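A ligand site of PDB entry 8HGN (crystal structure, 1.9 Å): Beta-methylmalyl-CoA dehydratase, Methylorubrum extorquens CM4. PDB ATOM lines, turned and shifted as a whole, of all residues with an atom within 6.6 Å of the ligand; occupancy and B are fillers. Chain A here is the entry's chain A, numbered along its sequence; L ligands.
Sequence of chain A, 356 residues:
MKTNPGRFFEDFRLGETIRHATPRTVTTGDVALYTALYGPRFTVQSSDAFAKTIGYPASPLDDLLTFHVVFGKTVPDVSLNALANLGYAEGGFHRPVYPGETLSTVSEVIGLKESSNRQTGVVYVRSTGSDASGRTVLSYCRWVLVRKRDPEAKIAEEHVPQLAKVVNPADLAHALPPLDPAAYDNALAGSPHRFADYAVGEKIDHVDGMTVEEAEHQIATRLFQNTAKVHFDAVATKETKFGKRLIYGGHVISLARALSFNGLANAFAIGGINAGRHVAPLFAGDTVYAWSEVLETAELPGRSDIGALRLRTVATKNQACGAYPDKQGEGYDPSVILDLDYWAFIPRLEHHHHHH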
ATOM      1  N   PHE A  71     -14.115  12.834 -21.266  1.00  0.00           N
ATOM      2  CA  PHE A  71     -15.578  12.596 -21.470  1.00  0.00           C
ATOM      3  C   PHE A  71     -16.357  13.858 -21.089  1.00  0.00           C
ATOM      4  O   PHE A  71     -17.231  14.317 -21.883  1.00  0.00           O
ATOM      5  CB  PHE A  71     -15.967  11.335 -20.694  1.00  0.00           C
ATOM      6  CG  PHE A  71     -17.407  10.903 -20.807  1.00  0.00           C
ATOM      7  CD1 PHE A  71     -18.450  11.698 -20.344  1.00  0.00           C
ATOM      8  CD2 PHE A  71     -17.720   9.685 -21.383  1.00  0.00           C
ATOM      9  CE1 PHE A  71     -19.761  11.250 -20.402  1.00  0.00           C
ATOM     10  CE2 PHE A  71     -19.036   9.251 -21.444  1.00  0.00           C
ATOM     11  CZ  PHE A  71     -20.050  10.046 -20.994  1.00  0.00           C
ATOM     12  N   THR A  74     -16.867  16.738 -23.471  1.00  0.00           N
ATOM     13  CA  THR A  74     -17.780  16.423 -24.612  1.00  0.00           C
ATOM     14  C   THR A  74     -19.227  16.594 -24.160  1.00  0.00           C
ATOM     15  O   THR A  74     -20.122  16.610 -25.020  1.00  0.00           O
ATOM     16  CB  THR A  74     -17.592  15.005 -25.176  1.00  0.00           C
ATOM     17  OG1 THR A  74     -18.148  14.053 -24.264  1.00  0.00           O
ATOM     18  CG2 THR A  74     -16.151  14.620 -25.432  1.00  0.00           C
ATOM     19  N   VAL A  75     -19.510  16.616 -22.853  1.00  0.00           N
ATOM     20  CA  VAL A  75     -20.934  16.449 -22.467  1.00  0.00           C
ATOM     21  C   VAL A  75     -21.772  17.642 -22.929  1.00  0.00           C
ATOM     22  O   VAL A  75     -22.803  17.449 -23.550  1.00  0.00           O
ATOM     23  CB  VAL A  75     -21.113  16.043 -21.000  1.00  0.00           C
ATOM     24  CG1 VAL A  75     -22.564  16.105 -20.570  1.00  0.00           C
ATOM     25  CG2 VAL A  75     -20.542  14.636 -20.754  1.00  0.00           C
ATOM     26  N   VAL A  78     -22.737  16.995 -26.731  1.00  0.00           N
ATOM     27  CA  VAL A  78     -23.216  15.653 -27.150  1.00  0.00           C
ATOM     28  C   VAL A  78     -24.399  15.201 -26.279  1.00  0.00           C
ATOM     29  O   VAL A  78     -25.457  14.937 -26.843  1.00  0.00           O
ATOM     30  CB  VAL A  78     -22.050  14.652 -27.146  1.00  0.00           C
ATOM     31  CG1 VAL A  78     -22.474  13.252 -27.515  1.00  0.00           C
ATOM     32  CG2 VAL A  78     -20.930  15.100 -28.054  1.00  0.00           C
ATOM     33  N   SER A  79     -24.234  15.163 -24.953  1.00  0.00           N
ATOM     34  CA  SER A  79     -25.060  14.387 -23.991  1.00  0.00           C
ATOM     35  C   SER A  79     -25.652  15.273 -22.880  1.00  0.00           C
ATOM     36  O   SER A  79     -26.119  14.739 -21.876  1.00  0.00           O
ATOM     37  CB  SER A  79     -24.204  13.264 -23.421  1.00  0.00           C
ATOM     38  OG  SER A  79     -22.895  13.743 -23.072  1.00  0.00           O
ATOM     39  N   LEU A  80     -25.650  16.596 -23.042  1.00  0.00           N
ATOM     40  CA  LEU A  80     -26.288  17.513 -22.060  1.00  0.00           C
ATOM     41  C   LEU A  80     -27.719  17.067 -21.855  1.00  0.00           C
ATOM     42  O   LEU A  80     -28.204  17.138 -20.704  1.00  0.00           O
ATOM     43  CB  LEU A  80     -26.229  18.939 -22.630  1.00  0.00           C
ATOM     44  CG  LEU A  80     -27.043  19.978 -21.896  1.00  0.00           C
ATOM     45  CD1 LEU A  80     -26.656  20.055 -20.428  1.00  0.00           C
ATOM     46  CD2 LEU A  80     -26.873  21.333 -22.574  1.00  0.00           C
ATOM     47  N   ALA A  82     -28.956  13.965 -22.610  1.00  0.00           N
ATOM     48  CA  ALA A  82     -28.979  12.493 -22.570  1.00  0.00           C
ATOM     49  C   ALA A  82     -29.907  12.007 -21.455  1.00  0.00           C
ATOM     50  O   ALA A  82     -30.092  12.740 -20.423  1.00  0.00           O
ATOM     51  CB  ALA A  82     -27.570  11.958 -22.384  1.00  0.00           C
ATOM     52  N   LEU A  83     -30.504  10.841 -21.674  1.00  0.00           N
ATOM     53  CA  LEU A  83     -31.231  10.037 -20.663  1.00  0.00           C
ATOM     54  C   LEU A  83     -30.290   8.959 -20.091  1.00  0.00           C
ATOM     55  O   LEU A  83     -30.463   8.609 -18.960  1.00  0.00           O
ATOM     56  CB  LEU A  83     -32.442   9.377 -21.324  1.00  0.00           C
ATOM     57  CG  LEU A  83     -33.462  10.333 -21.928  1.00  0.00           C
ATOM     58  CD1 LEU A  83     -34.525   9.556 -22.697  1.00  0.00           C
ATOM     59  CD2 LEU A  83     -34.099  11.193 -20.854  1.00  0.00           C
ATOM     60  N   ALA A  84     -29.365   8.420 -20.871  1.00  0.00           N
ATOM     61  CA  ALA A  84     -28.354   7.452 -20.351  1.00  0.00           C
ATOM     62  C   ALA A  84     -27.258   7.209 -21.381  1.00  0.00           C
ATOM     63  O   ALA A  84     -27.584   7.009 -22.581  1.00  0.00           O
ATOM     64  CB  ALA A  84     -29.002   6.152 -19.987  1.00  0.00           C
ATOM     65  N   ASN A  85     -26.012   7.158 -20.925  1.00  0.00           N
ATOM     66  CA  ASN A  85     -24.859   6.691 -21.704  1.00  0.00           C
ATOM     67  C   ASN A  85     -24.867   5.164 -21.672  1.00  0.00           C
ATOM     68  O   ASN A  85     -25.181   4.547 -20.606  1.00  0.00           O
ATOM     69  CB  ASN A  85     -23.617   7.390 -21.191  1.00  0.00           C
ATOM     70  CG  ASN A  85     -22.392   6.992 -21.984  1.00  0.00           C
ATOM     71  OD1 ASN A  85     -22.300   7.317 -23.158  1.00  0.00           O
ATOM     72  ND2 ASN A  85     -21.453   6.354 -21.311  1.00  0.00           N
ATOM     73  N   LEU A  86     -24.610   4.519 -22.811  1.00  0.00           N
ATOM     74  CA  LEU A  86     -24.963   3.096 -22.993  1.00  0.00           C
ATOM     75  C   LEU A  86     -23.721   2.216 -23.087  1.00  0.00           C
ATOM     76  O   LEU A  86     -23.717   1.127 -22.455  1.00  0.00           O
ATOM     77  CB  LEU A  86     -25.833   2.987 -24.248  1.00  0.00           C
ATOM     78  CG  LEU A  86     -27.182   3.715 -24.167  1.00  0.00           C
ATOM     79  CD1 LEU A  86     -27.926   3.540 -25.469  1.00  0.00           C
ATOM     80  CD2 LEU A  86     -28.039   3.221 -23.001  1.00  0.00           C
ATOM     81  N   TYR A  88     -19.272   1.629 -24.713  1.00  0.00           N
ATOM     82  CA  TYR A  88     -17.957   2.082 -25.239  1.00  0.00           C
ATOM     83  C   TYR A  88     -17.374   0.975 -26.129  1.00  0.00           C
ATOM     84  O   TYR A  88     -17.715  -0.235 -25.925  1.00  0.00           O
ATOM     85  CB  TYR A  88     -16.994   2.385 -24.092  1.00  0.00           C
ATOM     86  CG  TYR A  88     -17.577   3.161 -22.919  1.00  0.00           C
ATOM     87  CD1 TYR A  88     -17.414   4.527 -22.853  1.00  0.00           C
ATOM     88  CD2 TYR A  88     -18.273   2.549 -21.892  1.00  0.00           C
ATOM     89  CE1 TYR A  88     -17.920   5.264 -21.800  1.00  0.00           C
ATOM     90  CE2 TYR A  88     -18.790   3.262 -20.825  1.00  0.00           C
ATOM     91  CZ  TYR A  88     -18.606   4.640 -20.788  1.00  0.00           C
ATOM     92  OH  TYR A  88     -19.091   5.410 -19.776  1.00  0.00           O
ATOM     93  N   ARG A 142     -18.059   5.998 -27.785  1.00  0.00           N
ATOM     94  CA  ARG A 142     -19.233   5.760 -26.911  1.00  0.00           C
ATOM     95  C   ARG A 142     -20.522   6.023 -27.700  1.00  0.00           C
ATOM     96  O   ARG A 142     -20.475   6.728 -28.765  1.00  0.00           O
ATOM     97  CB  ARG A 142     -19.155   6.646 -25.666  1.00  0.00           C
ATOM     98  CG  ARG A 142     -19.093   8.141 -25.963  1.00  0.00           C
ATOM     99  CD  ARG A 142     -20.033   8.835 -25.024  1.00  0.00           C
ATOM    100  NE  ARG A 142     -19.921  10.271 -24.908  1.00  0.00           N
ATOM    101  CZ  ARG A 142     -20.834  11.037 -24.291  1.00  0.00           C
ATOM    102  NH1 ARG A 142     -20.694  12.347 -24.254  1.00  0.00           N
ATOM    103  NH2 ARG A 142     -21.854  10.478 -23.688  1.00  0.00           N
ATOM    104  N   VAL A 144     -24.739   7.017 -26.594  1.00  0.00           N
ATOM    105  CA  VAL A 144     -25.591   7.570 -25.509  1.00  0.00           C
ATOM    106  C   VAL A 144     -26.989   7.809 -26.098  1.00  0.00           C
ATOM    107  O   VAL A 144     -27.063   8.322 -27.226  1.00  0.00           O
ATOM    108  CB  VAL A 144     -24.907   8.853 -24.971  1.00  0.00           C
ATOM    109  CG1 VAL A 144     -24.506   9.778 -26.114  1.00  0.00           C
ATOM    110  CG2 VAL A 144     -25.738   9.591 -23.910  1.00  0.00           C
ATOM    111  N   THR A 221     -19.407  14.511 -10.598  1.00  0.00           N
ATOM    112  CA  THR A 221     -19.883  14.775 -11.963  1.00  0.00           C
ATOM    113  C   THR A 221     -19.506  16.202 -12.296  1.00  0.00           C
ATOM    114  O   THR A 221     -18.986  16.404 -13.404  1.00  0.00           O
ATOM    115  CB  THR A 221     -21.376  14.488 -12.173  1.00  0.00           C
ATOM    116  OG1 THR A 221     -21.571  13.131 -11.776  1.00  0.00           O
ATOM    117  CG2 THR A 221     -21.757  14.716 -13.626  1.00  0.00           C
ATOM    118  N   ASN A 226     -19.026  17.709 -16.341  1.00  0.00           N
ATOM    119  CA  ASN A 226     -20.056  16.924 -17.079  1.00  0.00           C
ATOM    120  C   ASN A 226     -21.410  17.501 -16.650  1.00  0.00           C
ATOM    121  O   ASN A 226     -21.663  17.562 -15.424  1.00  0.00           O
ATOM    122  CB  ASN A 226     -19.886  15.437 -16.763  1.00  0.00           C
ATOM    123  CG  ASN A 226     -21.053  14.528 -17.092  1.00  0.00           C
ATOM    124  OD1 ASN A 226     -22.200  14.946 -17.256  1.00  0.00           O
ATOM    125  ND2 ASN A 226     -20.757  13.244 -17.175  1.00  0.00           N
ATOM    126  N   THR A 227     -22.197  17.988 -17.603  1.00  0.00           N
ATOM    127  CA  THR A 227     -23.369  18.865 -17.346  1.00  0.00           C
ATOM    128  C   THR A 227     -24.693  18.114 -17.522  1.00  0.00           C
ATOM    129  O   THR A 227     -25.733  18.784 -17.375  1.00  0.00           O
ATOM    130  CB  THR A 227     -23.263  20.117 -18.212  1.00  0.00           C
ATOM    131  OG1 THR A 227     -23.061  19.601 -19.510  1.00  0.00           O
ATOM    132  CG2 THR A 227     -22.114  21.038 -17.852  1.00  0.00           C
ATOM    133  N   ALA A 228     -24.706  16.804 -17.758  1.00  0.00           N
ATOM    134  CA  ALA A 228     -25.933  16.088 -18.199  1.00  0.00           C
ATOM    135  C   ALA A 228     -27.021  16.312 -17.160  1.00  0.00           C
ATOM    136  O   ALA A 228     -26.819  15.853 -16.020  1.00  0.00           O
ATOM    137  CB  ALA A 228     -25.698  14.612 -18.401  1.00  0.00           C
ATOM    138  N   VAL A 230     -29.812  15.233 -16.216  1.00  0.00           N
ATOM    139  CA  VAL A 230     -30.363  14.052 -15.498  1.00  0.00           C
ATOM    140  C   VAL A 230     -29.552  13.713 -14.226  1.00  0.00           C
ATOM    141  O   VAL A 230     -30.100  13.068 -13.286  1.00  0.00           O
ATOM    142  CB  VAL A 230     -30.487  12.883 -16.496  1.00  0.00           C
ATOM    143  CG1 VAL A 230     -29.981  11.551 -15.976  1.00  0.00           C
ATOM    144  CG2 VAL A 230     -31.896  12.733 -17.024  1.00  0.00           C
ATOM    145  N   HIS A 231     -28.311  14.196 -14.106  1.00  0.00           N
ATOM    146  CA  HIS A 231     -27.477  14.019 -12.876  1.00  0.00           C
ATOM    147  C   HIS A 231     -27.919  14.967 -11.745  1.00  0.00           C
ATOM    148  O   HIS A 231     -27.746  14.630 -10.570  1.00  0.00           O
ATOM    149  CB  HIS A 231     -25.993  14.166 -13.227  1.00  0.00           C
ATOM    150  CG  HIS A 231     -25.556  13.197 -14.250  1.00  0.00           C
ATOM    151  ND1 HIS A 231     -25.995  11.883 -14.270  1.00  0.00           N
ATOM    152  CD2 HIS A 231     -24.793  13.349 -15.360  1.00  0.00           C
ATOM    153  CE1 HIS A 231     -25.464  11.253 -15.312  1.00  0.00           C
ATOM    154  NE2 HIS A 231     -24.714  12.118 -15.986  1.00  0.00           N
ATOM    155  N   LEU A 246     -30.285  10.287 -12.113  1.00  0.00           N
ATOM    156  CA  LEU A 246     -29.463   9.119 -12.544  1.00  0.00           C
ATOM    157  C   LEU A 246     -28.016   9.456 -12.208  1.00  0.00           C
ATOM    158  O   LEU A 246     -27.575  10.556 -12.568  1.00  0.00           O
ATOM    159  CB  LEU A 246     -29.605   8.852 -14.047  1.00  0.00           C
ATOM    160  CG  LEU A 246     -28.497   8.021 -14.703  1.00  0.00           C
ATOM    161  CD1 LEU A 246     -28.698   6.553 -14.409  1.00  0.00           C
ATOM    162  CD2 LEU A 246     -28.411   8.241 -16.202  1.00  0.00           C
ATOM    163  N   ILE A 247     -27.314   8.514 -11.563  1.00  0.00           N
ATOM    164  CA  ILE A 247     -25.861   8.619 -11.236  1.00  0.00           C
ATOM    165  C   ILE A 247     -25.073   8.407 -12.511  1.00  0.00           C
ATOM    166  O   ILE A 247     -25.315   7.425 -13.221  1.00  0.00           O
ATOM    167  CB  ILE A 247     -25.410   7.631 -10.149  1.00  0.00           C
ATOM    168  CG1 ILE A 247     -26.143   7.873  -8.840  1.00  0.00           C
ATOM    169  CG2 ILE A 247     -23.880   7.743 -10.002  1.00  0.00           C
ATOM    170  CD1 ILE A 247     -25.821   6.906  -7.765  1.00  0.00           C
ATOM    171  N   TYR A 248     -24.120   9.300 -12.750  1.00  0.00           N
ATOM    172  CA  TYR A 248     -23.133   9.216 -13.836  1.00  0.00           C
ATOM    173  C   TYR A 248     -22.690   7.763 -14.009  1.00  0.00           C
ATOM    174  O   TYR A 248     -22.221   7.163 -13.000  1.00  0.00           O
ATOM    175  CB  TYR A 248     -21.978  10.170 -13.535  1.00  0.00           C
ATOM    176  CG  TYR A 248     -20.832  10.123 -14.517  1.00  0.00           C
ATOM    177  CD1 TYR A 248     -19.522  10.159 -14.085  1.00  0.00           C
ATOM    178  CD2 TYR A 248     -21.063  10.028 -15.878  1.00  0.00           C
ATOM    179  CE1 TYR A 248     -18.473  10.079 -14.988  1.00  0.00           C
ATOM    180  CE2 TYR A 248     -20.035   9.962 -16.800  1.00  0.00           C
ATOM    181  CZ  TYR A 248     -18.735  10.003 -16.359  1.00  0.00           C
ATOM    182  OH  TYR A 248     -17.750   9.949 -17.304  1.00  0.00           O
ATOM    183  N   GLY A 249     -22.864   7.186 -15.210  1.00  0.00           N
ATOM    184  CA  GLY A 249     -22.340   5.846 -15.504  1.00  0.00           C
ATOM    185  C   GLY A 249     -20.860   5.711 -15.123  1.00  0.00           C
ATOM    186  O   GLY A 249     -20.451   4.637 -14.541  1.00  0.00           O
ATOM    187  N   GLY A 250     -20.052   6.708 -15.451  1.00  0.00           N
ATOM    188  CA  GLY A 250     -18.599   6.691 -15.145  1.00  0.00           C
ATOM    189  C   GLY A 250     -18.325   6.490 -13.658  1.00  0.00           C
ATOM    190  O   GLY A 250     -17.274   5.923 -13.311  1.00  0.00           O
ATOM    191  N   HIS A 251     -19.243   6.943 -12.796  1.00  0.00           N
ATOM    192  CA  HIS A 251     -19.090   6.833 -11.328  1.00  0.00           C
ATOM    193  C   HIS A 251     -19.022   5.356 -10.939  1.00  0.00           C
ATOM    194  O   HIS A 251     -18.214   4.994 -10.081  1.00  0.00           O
ATOM    195  CB  HIS A 251     -20.217   7.556 -10.633  1.00  0.00           C
ATOM    196  CG  HIS A 251     -19.884   7.924  -9.222  1.00  0.00           C
ATOM    197  ND1 HIS A 251     -20.158   7.081  -8.152  1.00  0.00           N
ATOM    198  CD2 HIS A 251     -19.384   9.051  -8.701  1.00  0.00           C
ATOM    199  CE1 HIS A 251     -19.804   7.686  -7.050  1.00  0.00           C
ATOM    200  NE2 HIS A 251     -19.321   8.866  -7.361  1.00  0.00           N
ATOM    201  N   HIS A 278     -23.223   0.027 -20.058  1.00  0.00           N
ATOM    202  CA  HIS A 278     -24.096   0.399 -18.905  1.00  0.00           C
ATOM    203  C   HIS A 278     -25.410  -0.378 -18.996  1.00  0.00           C
ATOM    204  O   HIS A 278     -26.310   0.054 -19.758  1.00  0.00           O
ATOM    205  CB  HIS A 278     -24.289   1.914 -18.815  1.00  0.00           C
ATOM    206  CG  HIS A 278     -23.000   2.643 -18.598  1.00  0.00           C
ATOM    207  ND1 HIS A 278     -22.296   2.549 -17.428  1.00  0.00           N
ATOM    208  CD2 HIS A 278     -22.293   3.455 -19.407  1.00  0.00           C
ATOM    209  CE1 HIS A 278     -21.219   3.291 -17.519  1.00  0.00           C
ATOM    210  NE2 HIS A 278     -21.198   3.868 -18.702  1.00  0.00           N
HETATM  211  C1  LIG L   1     -23.518  11.680 -20.549  1.00  0.00           C
HETATM  212  O1  LIG L   1     -23.544  10.858 -21.509  1.00  0.00           O
HETATM  213  O2  LIG L   1     -23.121  12.842 -20.616  1.00  0.00           O
HETATM  214  C2  LIG L   1     -23.999  11.211 -19.185  1.00  0.00           C
HETATM  215  O3  LIG L   1     -23.111  11.774 -18.241  1.00  0.00           O
HETATM  216  C3  LIG L   1     -24.047   9.677 -19.150  1.00  0.00           C
HETATM  217  C4  LIG L   1     -24.564   8.899 -17.948  1.00  0.00           C
HETATM  218  O4  LIG L   1     -25.586   8.173 -18.102  1.00  0.00           O
HETATM  219  O5  LIG L   1     -23.877   8.879 -16.944  1.00  0.00           O
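Phe 71 touches the ligand.
CG2 of Val 75 touches O2 of the ligand (3.1 Å).
CA of Ala 84 touches O4 of the ligand, 3.6 Å away.
Val 144 touches the ligand.
Ala 228 touches the ligand (CB to O2, 3.8 Å).
CD2 of Leu 246 touches O4 of the ligand (3.4 Å).
CA of Tyr 248 touches O5 of the ligand, at 3.2 Å.
Hydrophobic or aromatic side chains that line the ligand: Phe 71, Val 75, Val 144, Ala 228, His 231, Leu 246 and Tyr 248.
The side-chain hydroxyl of Thr 74 is in hydrogen-bond range of the guanidinium group of Arg 142 (3.1 Å).
N of Leu 80 sits at hydrogen-bond distance from O of Val 75 (3.0 Å).
The backbone carbonyl oxygen (O) of Phe 71 lies within hydrogen-bond range of the side-chain hydroxyl (OG1) of Thr 74, 2.6 Å away.
The guanidinium group of Arg 142 lies within hydrogen-bond range of the side-chain amide oxygen of Asn 85 (3.2 Å).
The backbone NH (N) of Asn 226 sits at hydrogen-bond distance from the backbone carbonyl oxygen (O) of Thr 221 (3.2 Å).
The backbone carbonyl oxygen (O) of Leu 246 lies within hydrogen-bond range of a ring nitrogen (ND1) of His 231, at 2.7 Å.
The side-chain amide nitrogen (ND2) of Asn 85 lies within hydrogen-bond range of the side-chain hydroxyl (OH) of Tyr 88 (3.0 Å).
The side-chain amide oxygen of Asn 226 is in hydrogen-bond range of the backbone NH of Ala 228, 3.2 Å away.
N of Asn 85 sits at hydrogen-bond distance from O4 of the ligand.
O3 of the ligand is in hydrogen-bond range of NE2 of His 231 (2.8 Å).
The side-chain amide nitrogen (ND2) of Asn 226 lies within hydrogen-bond range of an oxygen (O3) of the ligand.
The backbone NH of Gly 249 lies within hydrogen-bond range of an oxygen (O5) of the ligand.
NH2 of Arg 142 is in salt-bridge range of O1 of the ligand (2.8 Å).
OG of Ser 79 is in hydrogen-bond range of O2 of the ligand.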
